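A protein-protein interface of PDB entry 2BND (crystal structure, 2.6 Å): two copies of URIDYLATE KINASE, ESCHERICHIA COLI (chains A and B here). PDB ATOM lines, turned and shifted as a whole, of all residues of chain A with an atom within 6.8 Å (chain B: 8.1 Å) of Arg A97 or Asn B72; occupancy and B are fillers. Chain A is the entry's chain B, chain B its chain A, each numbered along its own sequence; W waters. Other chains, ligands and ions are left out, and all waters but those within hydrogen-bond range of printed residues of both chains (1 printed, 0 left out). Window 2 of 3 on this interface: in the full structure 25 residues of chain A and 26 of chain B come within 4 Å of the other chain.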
ATOM      1  N   ALA A  31      29.487 -15.754  20.982  1.00  0.00           N
ATOM      2  CA  ALA A  31      28.495 -15.862  19.927  1.00  0.00           C
ATOM      3  C   ALA A  31      27.422 -14.778  19.983  1.00  0.00           C
ATOM      4  O   ALA A  31      27.077 -14.185  18.957  1.00  0.00           O
ATOM      5  CB  ALA A  31      27.833 -17.224  19.993  1.00  0.00           C
ATOM      6  N   LEU A  34      28.496 -11.406  18.821  1.00  0.00           N
ATOM      7  CA  LEU A  34      28.633 -11.487  17.384  1.00  0.00           C
ATOM      8  C   LEU A  34      27.292 -11.323  16.696  1.00  0.00           C
ATOM      9  O   LEU A  34      27.167 -10.532  15.759  1.00  0.00           O
ATOM     10  CB  LEU A  34      29.253 -12.826  16.995  1.00  0.00           C
ATOM     11  CG  LEU A  34      30.654 -12.714  16.399  1.00  0.00           C
ATOM     12  CD1 LEU A  34      31.555 -11.906  17.322  1.00  0.00           C
ATOM     13  CD2 LEU A  34      31.210 -14.098  16.176  1.00  0.00           C
ATOM     14  N   ASP A  35      26.294 -12.075  17.156  1.00  0.00           N
ATOM     15  CA  ASP A  35      24.957 -12.005  16.574  1.00  0.00           C
ATOM     16  C   ASP A  35      24.377 -10.597  16.693  1.00  0.00           C
ATOM     17  O   ASP A  35      23.640 -10.140  15.812  1.00  0.00           O
ATOM     18  CB  ASP A  35      24.017 -12.977  17.280  1.00  0.00           C
ATOM     19  CG  ASP A  35      24.220 -14.413  16.854  1.00  0.00           C
ATOM     20  OD1 ASP A  35      23.729 -15.301  17.580  1.00  0.00           O
ATOM     21  OD2 ASP A  35      24.848 -14.658  15.800  1.00  0.00           O
ATOM     22  N   ALA A  38      26.069  -8.088  14.198  1.00  0.00           N
ATOM     23  CA  ALA A  38      25.635  -8.322  12.826  1.00  0.00           C
ATOM     24  C   ALA A  38      24.353  -7.523  12.634  1.00  0.00           C
ATOM     25  O   ALA A  38      24.144  -6.868  11.607  1.00  0.00           O
ATOM     26  CB  ALA A  38      25.373  -9.809  12.585  1.00  0.00           C
ATOM     27  N   GLN A  39      23.498  -7.565  13.645  1.00  0.00           N
ATOM     28  CA  GLN A  39      22.246  -6.833  13.580  1.00  0.00           C
ATOM     29  C   GLN A  39      22.476  -5.326  13.469  1.00  0.00           C
ATOM     30  O   GLN A  39      21.912  -4.671  12.597  1.00  0.00           O
ATOM     31  CB  GLN A  39      21.387  -7.152  14.806  1.00  0.00           C
ATOM     32  CG  GLN A  39      20.771  -8.552  14.769  1.00  0.00           C
ATOM     33  CD  GLN A  39      19.827  -8.735  13.596  1.00  0.00           C
ATOM     34  OE1 GLN A  39      18.926  -7.929  13.384  1.00  0.00           O
ATOM     35  NE2 GLN A  39      20.028  -9.797  12.831  1.00  0.00           N
ATOM     36  N   LYS A  42      23.888  -4.535  10.250  1.00  0.00           N
ATOM     37  CA  LYS A  42      22.859  -4.719   9.231  1.00  0.00           C
ATOM     38  C   LYS A  42      22.058  -3.429   9.043  1.00  0.00           C
ATOM     39  O   LYS A  42      21.773  -3.021   7.914  1.00  0.00           O
ATOM     40  CB  LYS A  42      21.926  -5.855   9.647  1.00  0.00           C
ATOM     41  CG  LYS A  42      20.807  -6.153   8.660  1.00  0.00           C
ATOM     42  CD  LYS A  42      20.011  -7.344   9.129  1.00  0.00           C
ATOM     43  CE  LYS A  42      19.046  -7.848   8.075  1.00  0.00           C
ATOM     44  NZ  LYS A  42      18.412  -9.121   8.528  1.00  0.00           N
ATOM     45  N   ALA A  90      34.478 -15.426  12.147  1.00  0.00           N
ATOM     46  CA  ALA A  90      33.257 -15.501  12.940  1.00  0.00           C
ATOM     47  C   ALA A  90      32.362 -14.281  12.706  1.00  0.00           C
ATOM     48  O   ALA A  90      31.141 -14.412  12.635  1.00  0.00           O
ATOM     49  CB  ALA A  90      33.594 -15.639  14.427  1.00  0.00           C
ATOM     50  N   ARG A  92      32.167 -12.502   9.970  1.00  0.00           N
ATOM     51  CA  ARG A  92      31.562 -12.623   8.648  1.00  0.00           C
ATOM     52  C   ARG A  92      30.405 -13.619   8.685  1.00  0.00           C
ATOM     53  O   ARG A  92      29.357 -13.413   8.063  1.00  0.00           O
ATOM     54  CB  ARG A  92      32.580 -13.096   7.618  1.00  0.00           C
ATOM     55  CG  ARG A  92      32.012 -13.193   6.204  1.00  0.00           C
ATOM     56  CD  ARG A  92      32.943 -13.961   5.307  1.00  0.00           C
ATOM     57  NE  ARG A  92      33.046 -15.351   5.728  1.00  0.00           N
ATOM     58  CZ  ARG A  92      33.890 -16.233   5.203  1.00  0.00           C
ATOM     59  NH1 ARG A  92      34.717 -15.870   4.235  1.00  0.00           N
ATOM     60  NH2 ARG A  92      33.890 -17.486   5.633  1.00  0.00           N
ATOM     61  N   ASP A  93      30.592 -14.705   9.420  1.00  0.00           N
ATOM     62  CA  ASP A  93      29.552 -15.712   9.494  1.00  0.00           C
ATOM     63  C   ASP A  93      28.302 -15.120  10.123  1.00  0.00           C
ATOM     64  O   ASP A  93      27.186 -15.369   9.660  1.00  0.00           O
ATOM     65  CB  ASP A  93      30.026 -16.914  10.299  1.00  0.00           C
ATOM     66  CG  ASP A  93      29.099 -18.101  10.150  1.00  0.00           C
ATOM     67  OD1 ASP A  93      28.881 -18.555   9.002  1.00  0.00           O
ATOM     68  OD2 ASP A  93      28.584 -18.574  11.180  1.00  0.00           O
ATOM     69  N   ALA A  94      28.488 -14.327  11.176  1.00  0.00           N
ATOM     70  CA  ALA A  94      27.343 -13.709  11.830  1.00  0.00           C
ATOM     71  C   ALA A  94      26.649 -12.807  10.808  1.00  0.00           C
ATOM     72  O   ALA A  94      25.426 -12.802  10.713  1.00  0.00           O
ATOM     73  CB  ALA A  94      27.787 -12.902  13.058  1.00  0.00           C
ATOM     74  N   LEU A  95      27.428 -12.054  10.036  1.00  0.00           N
ATOM     75  CA  LEU A  95      26.836 -11.192   9.030  1.00  0.00           C
ATOM     76  C   LEU A  95      26.036 -12.058   8.070  1.00  0.00           C
ATOM     77  O   LEU A  95      24.849 -11.830   7.858  1.00  0.00           O
ATOM     78  CB  LEU A  95      27.900 -10.423   8.240  1.00  0.00           C
ATOM     79  CG  LEU A  95      28.401  -9.018   8.618  1.00  0.00           C
ATOM     80  CD1 LEU A  95      27.334  -8.256   9.406  1.00  0.00           C
ATOM     81  CD2 LEU A  95      29.697  -9.121   9.390  1.00  0.00           C
ATOM     82  N   HIS A  96      26.684 -13.062   7.490  1.00  0.00           N
ATOM     83  CA  HIS A  96      25.994 -13.925   6.551  1.00  0.00           C
ATOM     84  C   HIS A  96      24.711 -14.537   7.120  1.00  0.00           C
ATOM     85  O   HIS A  96      23.667 -14.497   6.469  1.00  0.00           O
ATOM     86  CB  HIS A  96      26.946 -15.010   6.040  1.00  0.00           C
ATOM     87  CG  HIS A  96      27.973 -14.499   5.076  1.00  0.00           C
ATOM     88  ND1 HIS A  96      28.907 -15.315   4.474  1.00  0.00           N
ATOM     89  CD2 HIS A  96      28.204 -13.252   4.603  1.00  0.00           C
ATOM     90  CE1 HIS A  96      29.669 -14.592   3.672  1.00  0.00           C
ATOM     91  NE2 HIS A  96      29.262 -13.337   3.731  1.00  0.00           N
ATOM     92  N   ARG A  97      24.767 -15.086   8.330  1.00  0.00           N
ATOM     93  CA  ARG A  97      23.572 -15.674   8.909  1.00  0.00           C
ATOM     94  C   ARG A  97      22.497 -14.614   9.205  1.00  0.00           C
ATOM     95  O   ARG A  97      21.342 -14.948   9.493  1.00  0.00           O
ATOM     96  CB  ARG A  97      23.924 -16.481  10.166  1.00  0.00           C
ATOM     97  CG  ARG A  97      24.617 -17.816   9.857  1.00  0.00           C
ATOM     98  CD  ARG A  97      24.978 -18.629  11.115  1.00  0.00           C
ATOM     99  NE  ARG A  97      25.881 -17.903  12.014  1.00  0.00           N
ATOM    100  CZ  ARG A  97      25.476 -17.129  13.017  1.00  0.00           C
ATOM    101  NH1 ARG A  97      24.179 -16.984  13.263  1.00  0.00           N
ATOM    102  NH2 ARG A  97      26.362 -16.489  13.768  1.00  0.00           N
ATOM    103  N   ALA A  98      22.871 -13.338   9.134  1.00  0.00           N
ATOM    104  CA  ALA A  98      21.913 -12.251   9.347  1.00  0.00           C
ATOM    105  C   ALA A  98      21.495 -11.697   7.964  1.00  0.00           C
ATOM    106  O   ALA A  98      20.787 -10.683   7.855  1.00  0.00           O
ATOM    107  CB  ALA A  98      22.533 -11.141  10.217  1.00  0.00           C
ATOM    108  N   TYR A  99      21.949 -12.374   6.913  1.00  0.00           N
ATOM    109  CA  TYR A  99      21.607 -12.000   5.546  1.00  0.00           C
ATOM    110  C   TYR A  99      22.156 -10.626   5.179  1.00  0.00           C
ATOM    111  O   TYR A  99      21.443  -9.773   4.662  1.00  0.00           O
ATOM    112  CB  TYR A  99      20.079 -12.035   5.361  1.00  0.00           C
ATOM    113  CG  TYR A  99      19.443 -13.315   5.882  1.00  0.00           C
ATOM    114  CD1 TYR A  99      19.477 -14.498   5.132  1.00  0.00           C
ATOM    115  CD2 TYR A  99      18.877 -13.360   7.166  1.00  0.00           C
ATOM    116  CE1 TYR A  99      18.966 -15.704   5.652  1.00  0.00           C
ATOM    117  CE2 TYR A  99      18.369 -14.548   7.695  1.00  0.00           C
ATOM    118  CZ  TYR A  99      18.416 -15.719   6.939  1.00  0.00           C
ATOM    119  OH  TYR A  99      17.936 -16.900   7.486  1.00  0.00           O
ATOM    120  N   VAL A 100      23.434 -10.426   5.455  1.00  0.00           N
ATOM    121  CA  VAL A 100      24.102  -9.181   5.141  1.00  0.00           C
ATOM    122  C   VAL A 100      25.281  -9.511   4.239  1.00  0.00           C
ATOM    123  O   VAL A 100      26.115 -10.358   4.574  1.00  0.00           O
ATOM    124  CB  VAL A 100      24.608  -8.493   6.404  1.00  0.00           C
ATOM    125  CG1 VAL A 100      25.333  -7.235   6.036  1.00  0.00           C
ATOM    126  CG2 VAL A 100      23.434  -8.196   7.330  1.00  0.00           C
ATOM    127  N   GLY B  63      35.287 -26.922  15.469  1.00  0.00           N
ATOM    128  CA  GLY B  63      34.162 -26.578  14.620  1.00  0.00           C
ATOM    129  C   GLY B  63      32.811 -26.978  15.179  1.00  0.00           C
ATOM    130  O   GLY B  63      31.862 -26.201  15.129  1.00  0.00           O
ATOM    131  N   ALA B  64      32.711 -28.185  15.716  1.00  0.00           N
ATOM    132  CA  ALA B  64      31.441 -28.643  16.263  1.00  0.00           C
ATOM    133  C   ALA B  64      30.942 -27.693  17.346  1.00  0.00           C
ATOM    134  O   ALA B  64      29.806 -27.216  17.296  1.00  0.00           O
ATOM    135  CB  ALA B  64      31.586 -30.051  16.826  1.00  0.00           C
ATOM    136  N   LEU B  66      31.547 -24.615  17.939  1.00  0.00           N
ATOM    137  CA  LEU B  66      31.125 -23.326  17.414  1.00  0.00           C
ATOM    138  C   LEU B  66      29.785 -23.481  16.706  1.00  0.00           C
ATOM    139  O   LEU B  66      28.877 -22.660  16.862  1.00  0.00           O
ATOM    140  CB  LEU B  66      32.176 -22.793  16.445  1.00  0.00           C
ATOM    141  CG  LEU B  66      33.546 -22.487  17.055  1.00  0.00           C
ATOM    142  CD1 LEU B  66      34.593 -22.394  15.961  1.00  0.00           C
ATOM    143  CD2 LEU B  66      33.471 -21.189  17.857  1.00  0.00           C
ATOM    144  N   ALA B  67      29.661 -24.549  15.932  1.00  0.00           N
ATOM    145  CA  ALA B  67      28.428 -24.802  15.205  1.00  0.00           C
ATOM    146  C   ALA B  67      27.254 -24.786  16.186  1.00  0.00           C
ATOM    147  O   ALA B  67      26.212 -24.198  15.906  1.00  0.00           O
ATOM    148  CB  ALA B  67      28.517 -26.149  14.472  1.00  0.00           C
ATOM    149  N   LYS B  68      27.436 -25.411  17.345  1.00  0.00           N
ATOM    150  CA  LYS B  68      26.384 -25.455  18.354  1.00  0.00           C
ATOM    151  C   LYS B  68      25.999 -24.060  18.842  1.00  0.00           C
ATOM    152  O   LYS B  68      24.850 -23.811  19.189  1.00  0.00           O
ATOM    153  CB  LYS B  68      26.815 -26.319  19.543  1.00  0.00           C
ATOM    154  CG  LYS B  68      26.771 -27.811  19.252  1.00  0.00           C
ATOM    155  CD  LYS B  68      26.892 -28.645  20.518  1.00  0.00           C
ATOM    156  CE  LYS B  68      26.683 -30.119  20.213  1.00  0.00           C
ATOM    157  NZ  LYS B  68      26.740 -30.944  21.452  1.00  0.00           N
ATOM    158  N   ALA B  69      26.963 -23.152  18.873  1.00  0.00           N
ATOM    159  CA  ALA B  69      26.689 -21.792  19.302  1.00  0.00           C
ATOM    160  C   ALA B  69      25.904 -21.053  18.220  1.00  0.00           C
ATOM    161  O   ALA B  69      25.538 -19.898  18.409  1.00  0.00           O
ATOM    162  CB  ALA B  69      27.994 -21.063  19.604  1.00  0.00           C
ATOM    163  N   GLY B  70      25.663 -21.715  17.084  1.00  0.00           N
ATOM    164  CA  GLY B  70      24.895 -21.106  16.003  1.00  0.00           C
ATOM    165  C   GLY B  70      25.625 -20.815  14.698  1.00  0.00           C
ATOM    166  O   GLY B  70      24.994 -20.588  13.658  1.00  0.00           O
ATOM    167  N   MET B  71      26.953 -20.812  14.751  1.00  0.00           N
ATOM    168  CA  MET B  71      27.790 -20.540  13.583  1.00  0.00           C
ATOM    169  C   MET B  71      27.751 -21.677  12.551  1.00  0.00           C
ATOM    170  O   MET B  71      27.514 -22.835  12.905  1.00  0.00           O
ATOM    171  CB  MET B  71      29.231 -20.313  14.044  1.00  0.00           C
ATOM    172  CG  MET B  71      30.250 -20.090  12.939  1.00  0.00           C
ATOM    173  SD  MET B  71      31.926 -19.990  13.618  1.00  0.00           S
ATOM    174  CE  MET B  71      31.802 -18.469  14.521  1.00  0.00           C
ATOM    175  N   ASN B  72      27.977 -21.338  11.281  1.00  0.00           N
ATOM    176  CA  ASN B  72      27.998 -22.330  10.201  1.00  0.00           C
ATOM    177  C   ASN B  72      29.043 -23.410  10.480  1.00  0.00           C
ATOM    178  O   ASN B  72      30.169 -23.117  10.882  1.00  0.00           O
ATOM    179  CB  ASN B  72      28.330 -21.665   8.861  1.00  0.00           C
ATOM    180  CG  ASN B  72      27.096 -21.226   8.105  1.00  0.00           C
ATOM    181  OD1 ASN B  72      26.327 -22.060   7.625  1.00  0.00           O
ATOM    182  ND2 ASN B  72      26.894 -19.914   7.996  1.00  0.00           N
ATOM    183  N   ARG B  73      28.684 -24.663  10.248  1.00  0.00           N
ATOM    184  CA  ARG B  73      29.636 -25.722  10.505  1.00  0.00           C
ATOM    185  C   ARG B  73      30.936 -25.564   9.726  1.00  0.00           C
ATOM    186  O   ARG B  73      32.016 -25.691  10.296  1.00  0.00           O
ATOM    187  CB  ARG B  73      29.033 -27.095  10.203  1.00  0.00           C
ATOM    188  CG  ARG B  73      29.958 -28.221  10.631  1.00  0.00           C
ATOM    189  CD  ARG B  73      30.374 -28.030  12.089  1.00  0.00           C
ATOM    190  NE  ARG B  73      31.614 -28.723  12.421  1.00  0.00           N
ATOM    191  CZ  ARG B  73      31.728 -30.040  12.550  1.00  0.00           C
ATOM    192  NH1 ARG B  73      30.672 -30.825  12.379  1.00  0.00           N
ATOM    193  NH2 ARG B  73      32.906 -30.573  12.841  1.00  0.00           N
ATOM    194  N   VAL B  74      30.834 -25.284   8.429  1.00  0.00           N
ATOM    195  CA  VAL B  74      32.032 -25.143   7.606  1.00  0.00           C
ATOM    196  C   VAL B  74      32.967 -24.062   8.116  1.00  0.00           C
ATOM    197  O   VAL B  74      34.180 -24.266   8.196  1.00  0.00           O
ATOM    198  CB  VAL B  74      31.697 -24.835   6.126  1.00  0.00           C
ATOM    199  CG1 VAL B  74      32.994 -24.692   5.324  1.00  0.00           C
ATOM    200  CG2 VAL B  74      30.845 -25.955   5.537  1.00  0.00           C
ATOM    201  N   VAL B  75      32.412 -22.909   8.462  1.00  0.00           N
ATOM    202  CA  VAL B  75      33.241 -21.826   8.961  1.00  0.00           C
ATOM    203  C   VAL B  75      33.808 -22.203  10.331  1.00  0.00           C
ATOM    204  O   VAL B  75      34.925 -21.832  10.683  1.00  0.00           O
ATOM    205  CB  VAL B  75      32.435 -20.517   9.023  1.00  0.00           C
ATOM    206  CG1 VAL B  75      33.283 -19.399   9.607  1.00  0.00           C
ATOM    207  CG2 VAL B  75      31.976 -20.145   7.617  1.00  0.00           C
ATOM    208  N   GLY B  76      33.047 -22.964  11.099  1.00  0.00           N
ATOM    209  CA  GLY B  76      33.549 -23.384  12.388  1.00  0.00           C
ATOM    210  C   GLY B  76      34.800 -24.217  12.179  1.00  0.00           C
ATOM    211  O   GLY B  76      35.838 -23.966  12.789  1.00  0.00           O
ATOM    212  N   ASP B  77      34.703 -25.209  11.298  1.00  0.00           N
ATOM    213  CA  ASP B  77      35.828 -26.083  11.010  1.00  0.00           C
ATOM    214  C   ASP B  77      36.982 -25.310  10.370  1.00  0.00           C
ATOM    215  O   ASP B  77      38.135 -25.730  10.443  1.00  0.00           O
ATOM    216  CB  ASP B  77      35.389 -27.247  10.105  1.00  0.00           C
ATOM    217  CG  ASP B  77      34.562 -28.297  10.852  1.00  0.00           C
ATOM    218  OD1 ASP B  77      34.597 -28.307  12.101  1.00  0.00           O
ATOM    219  OD2 ASP B  77      33.883 -29.123  10.199  1.00  0.00           O
ATOM    220  N   HIS B  78      36.682 -24.181   9.736  1.00  0.00           N
ATOM    221  CA  HIS B  78      37.740 -23.391   9.134  1.00  0.00           C
ATOM    222  C   HIS B  78      38.537 -22.749  10.271  1.00  0.00           C
ATOM    223  O   HIS B  78      39.742 -22.939  10.381  1.00  0.00           O
ATOM    224  CB  HIS B  78      37.153 -22.327   8.191  1.00  0.00           C
ATOM    225  CG  HIS B  78      36.841 -22.840   6.816  1.00  0.00           C
ATOM    226  ND1 HIS B  78      36.195 -22.078   5.865  1.00  0.00           N
ATOM    227  CD2 HIS B  78      37.071 -24.043   6.236  1.00  0.00           C
ATOM    228  CE1 HIS B  78      36.039 -22.791   4.763  1.00  0.00           C
ATOM    229  NE2 HIS B  78      36.561 -23.987   4.963  1.00  0.00           N
ATOM    230  N   MET B  79      37.852 -22.000  11.124  1.00  0.00           N
ATOM    231  CA  MET B  79      38.490 -21.356  12.258  1.00  0.00           C
ATOM    232  C   MET B  79      39.266 -22.393  13.079  1.00  0.00           C
ATOM    233  O   MET B  79      40.369 -22.128  13.566  1.00  0.00           O
ATOM    234  CB  MET B  79      37.431 -20.706  13.143  1.00  0.00           C
ATOM    235  CG  MET B  79      36.747 -19.501  12.542  1.00  0.00           C
ATOM    236  SD  MET B  79      35.406 -18.962  13.615  1.00  0.00           S
ATOM    237  CE  MET B  79      36.249 -17.958  14.768  1.00  0.00           C
ATOM    238  N   PRO B 141      36.576 -29.426   5.979  1.00  0.00           N
ATOM    239  CA  PRO B 141      35.713 -29.395   7.165  1.00  0.00           C
ATOM    240  C   PRO B 141      35.194 -30.818   7.422  1.00  0.00           C
ATOM    241  O   PRO B 141      35.339 -31.702   6.572  1.00  0.00           O
ATOM    242  CB  PRO B 141      34.596 -28.441   6.746  1.00  0.00           C
ATOM    243  CG  PRO B 141      34.507 -28.659   5.273  1.00  0.00           C
ATOM    244  CD  PRO B 141      35.960 -28.678   4.867  1.00  0.00           C
ATOM    245  N   PHE B 142      34.598 -31.037   8.588  1.00  0.00           N
ATOM    246  CA  PHE B 142      34.054 -32.350   8.950  1.00  0.00           C
ATOM    247  C   PHE B 142      35.151 -33.390   9.114  1.00  0.00           C
ATOM    248  O   PHE B 142      34.944 -34.564   8.843  1.00  0.00           O
ATOM    249  CB  PHE B 142      33.054 -32.840   7.889  1.00  0.00           C
ATOM    250  CG  PHE B 142      31.982 -31.850   7.567  1.00  0.00           C
ATOM    251  CD1 PHE B 142      31.040 -31.488   8.524  1.00  0.00           C
ATOM    252  CD2 PHE B 142      31.940 -31.236   6.315  1.00  0.00           C
ATOM    253  CE1 PHE B 142      30.072 -30.523   8.242  1.00  0.00           C
ATOM    254  CE2 PHE B 142      30.976 -30.268   6.020  1.00  0.00           C
ATOM    255  CZ  PHE B 142      30.041 -29.911   6.989  1.00  0.00           C
HETATM  256  O   HOH W   1      35.700 -19.338   4.697  1.00  0.00           O
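Ala A31 touches Ala B69.
Ala A90 touches Met B71 (CB to CE, 3.4 Å).
Met B79 touches Ala A90.
NH2 of Arg A92 touches CG2 of Val B75, 3.8 Å away.
OD2 of Asp A93 touches CG of Met B71 (2.9 Å).
Asp A93 touches Val B75 (OD1 to CG2, 3.7 Å).
Met B71 touches Arg A97.
Asn B72 touches Arg A97 (ND2 to CG, 3.6 Å).
Of the printed residues of chain B, Ala A31 touches Ala B69 (3.9 Å).
Ala A38 touches none of the printed residues of chain B.
Of the printed residues of chain B, Ala A90 touches Met B71 and Met B79.
Of the printed residues of chain B, Arg A92 touches Val B75 (3.8 Å).
Arg A97 touches three residues of chain B.
Of the printed residues of chain A, Ala B69 touches Ala A31.
Of the printed residues of chain A, Asn B72 touches Asp A93 and Arg A97.
Asp B77 touches none of the printed residues of chain A.
The nearest residue of chain B that does not touch Arg A97 is Ala B69 (5.8 Å).
The nearest residue of chain A that does not touch Asn B72 is His A96 (5.3 Å).
The nearest printed residue of chain A that does not touch Ala B69 is Asp A35 (5.0 Å).
Hydrophobic or aromatic side chains of chain A within 4 Å of the printed part of chain B: Ala A31 and Ala A90.
Of the 18 printed residues of chain B, 6 touch a printed residue of chain A.
Hydrophobic or aromatic side chains of chain B that line the printed part of chain A: Ala B69, Met B71, Val B75 and Met B79.
Among the printed residues, 10 pairs touch across the chains.
Water W1 lies within hydrogen-bond range of the guanidinium group of Arg A92 (2.8 Å) and a ring nitrogen (ND1) of His B78 (3.0 Å).
The side-chain carboxylate of Asp A35 is in salt-bridge range of the guanidinium group of Arg A97 (3.1 Å).
OD2 of Asp A93 is in salt-bridge range of NE of Arg A97.
O of Leu B66 sits at hydrogen-bond distance from N of Met B71, at 3.4 Å.
The side-chain amide nitrogen (ND2) of Asn B72 lies within hydrogen-bond range of the side-chain carboxylate (OD1) of Asp A93 (2.6 Å).
NE of Arg A97 sits close to O of Gly B70, 3.3 Å away.
No position is printed for both chains.
Of the 10 pairs that touch across the chains among the printed residues, none has its exchanged pair printed and touching as well.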
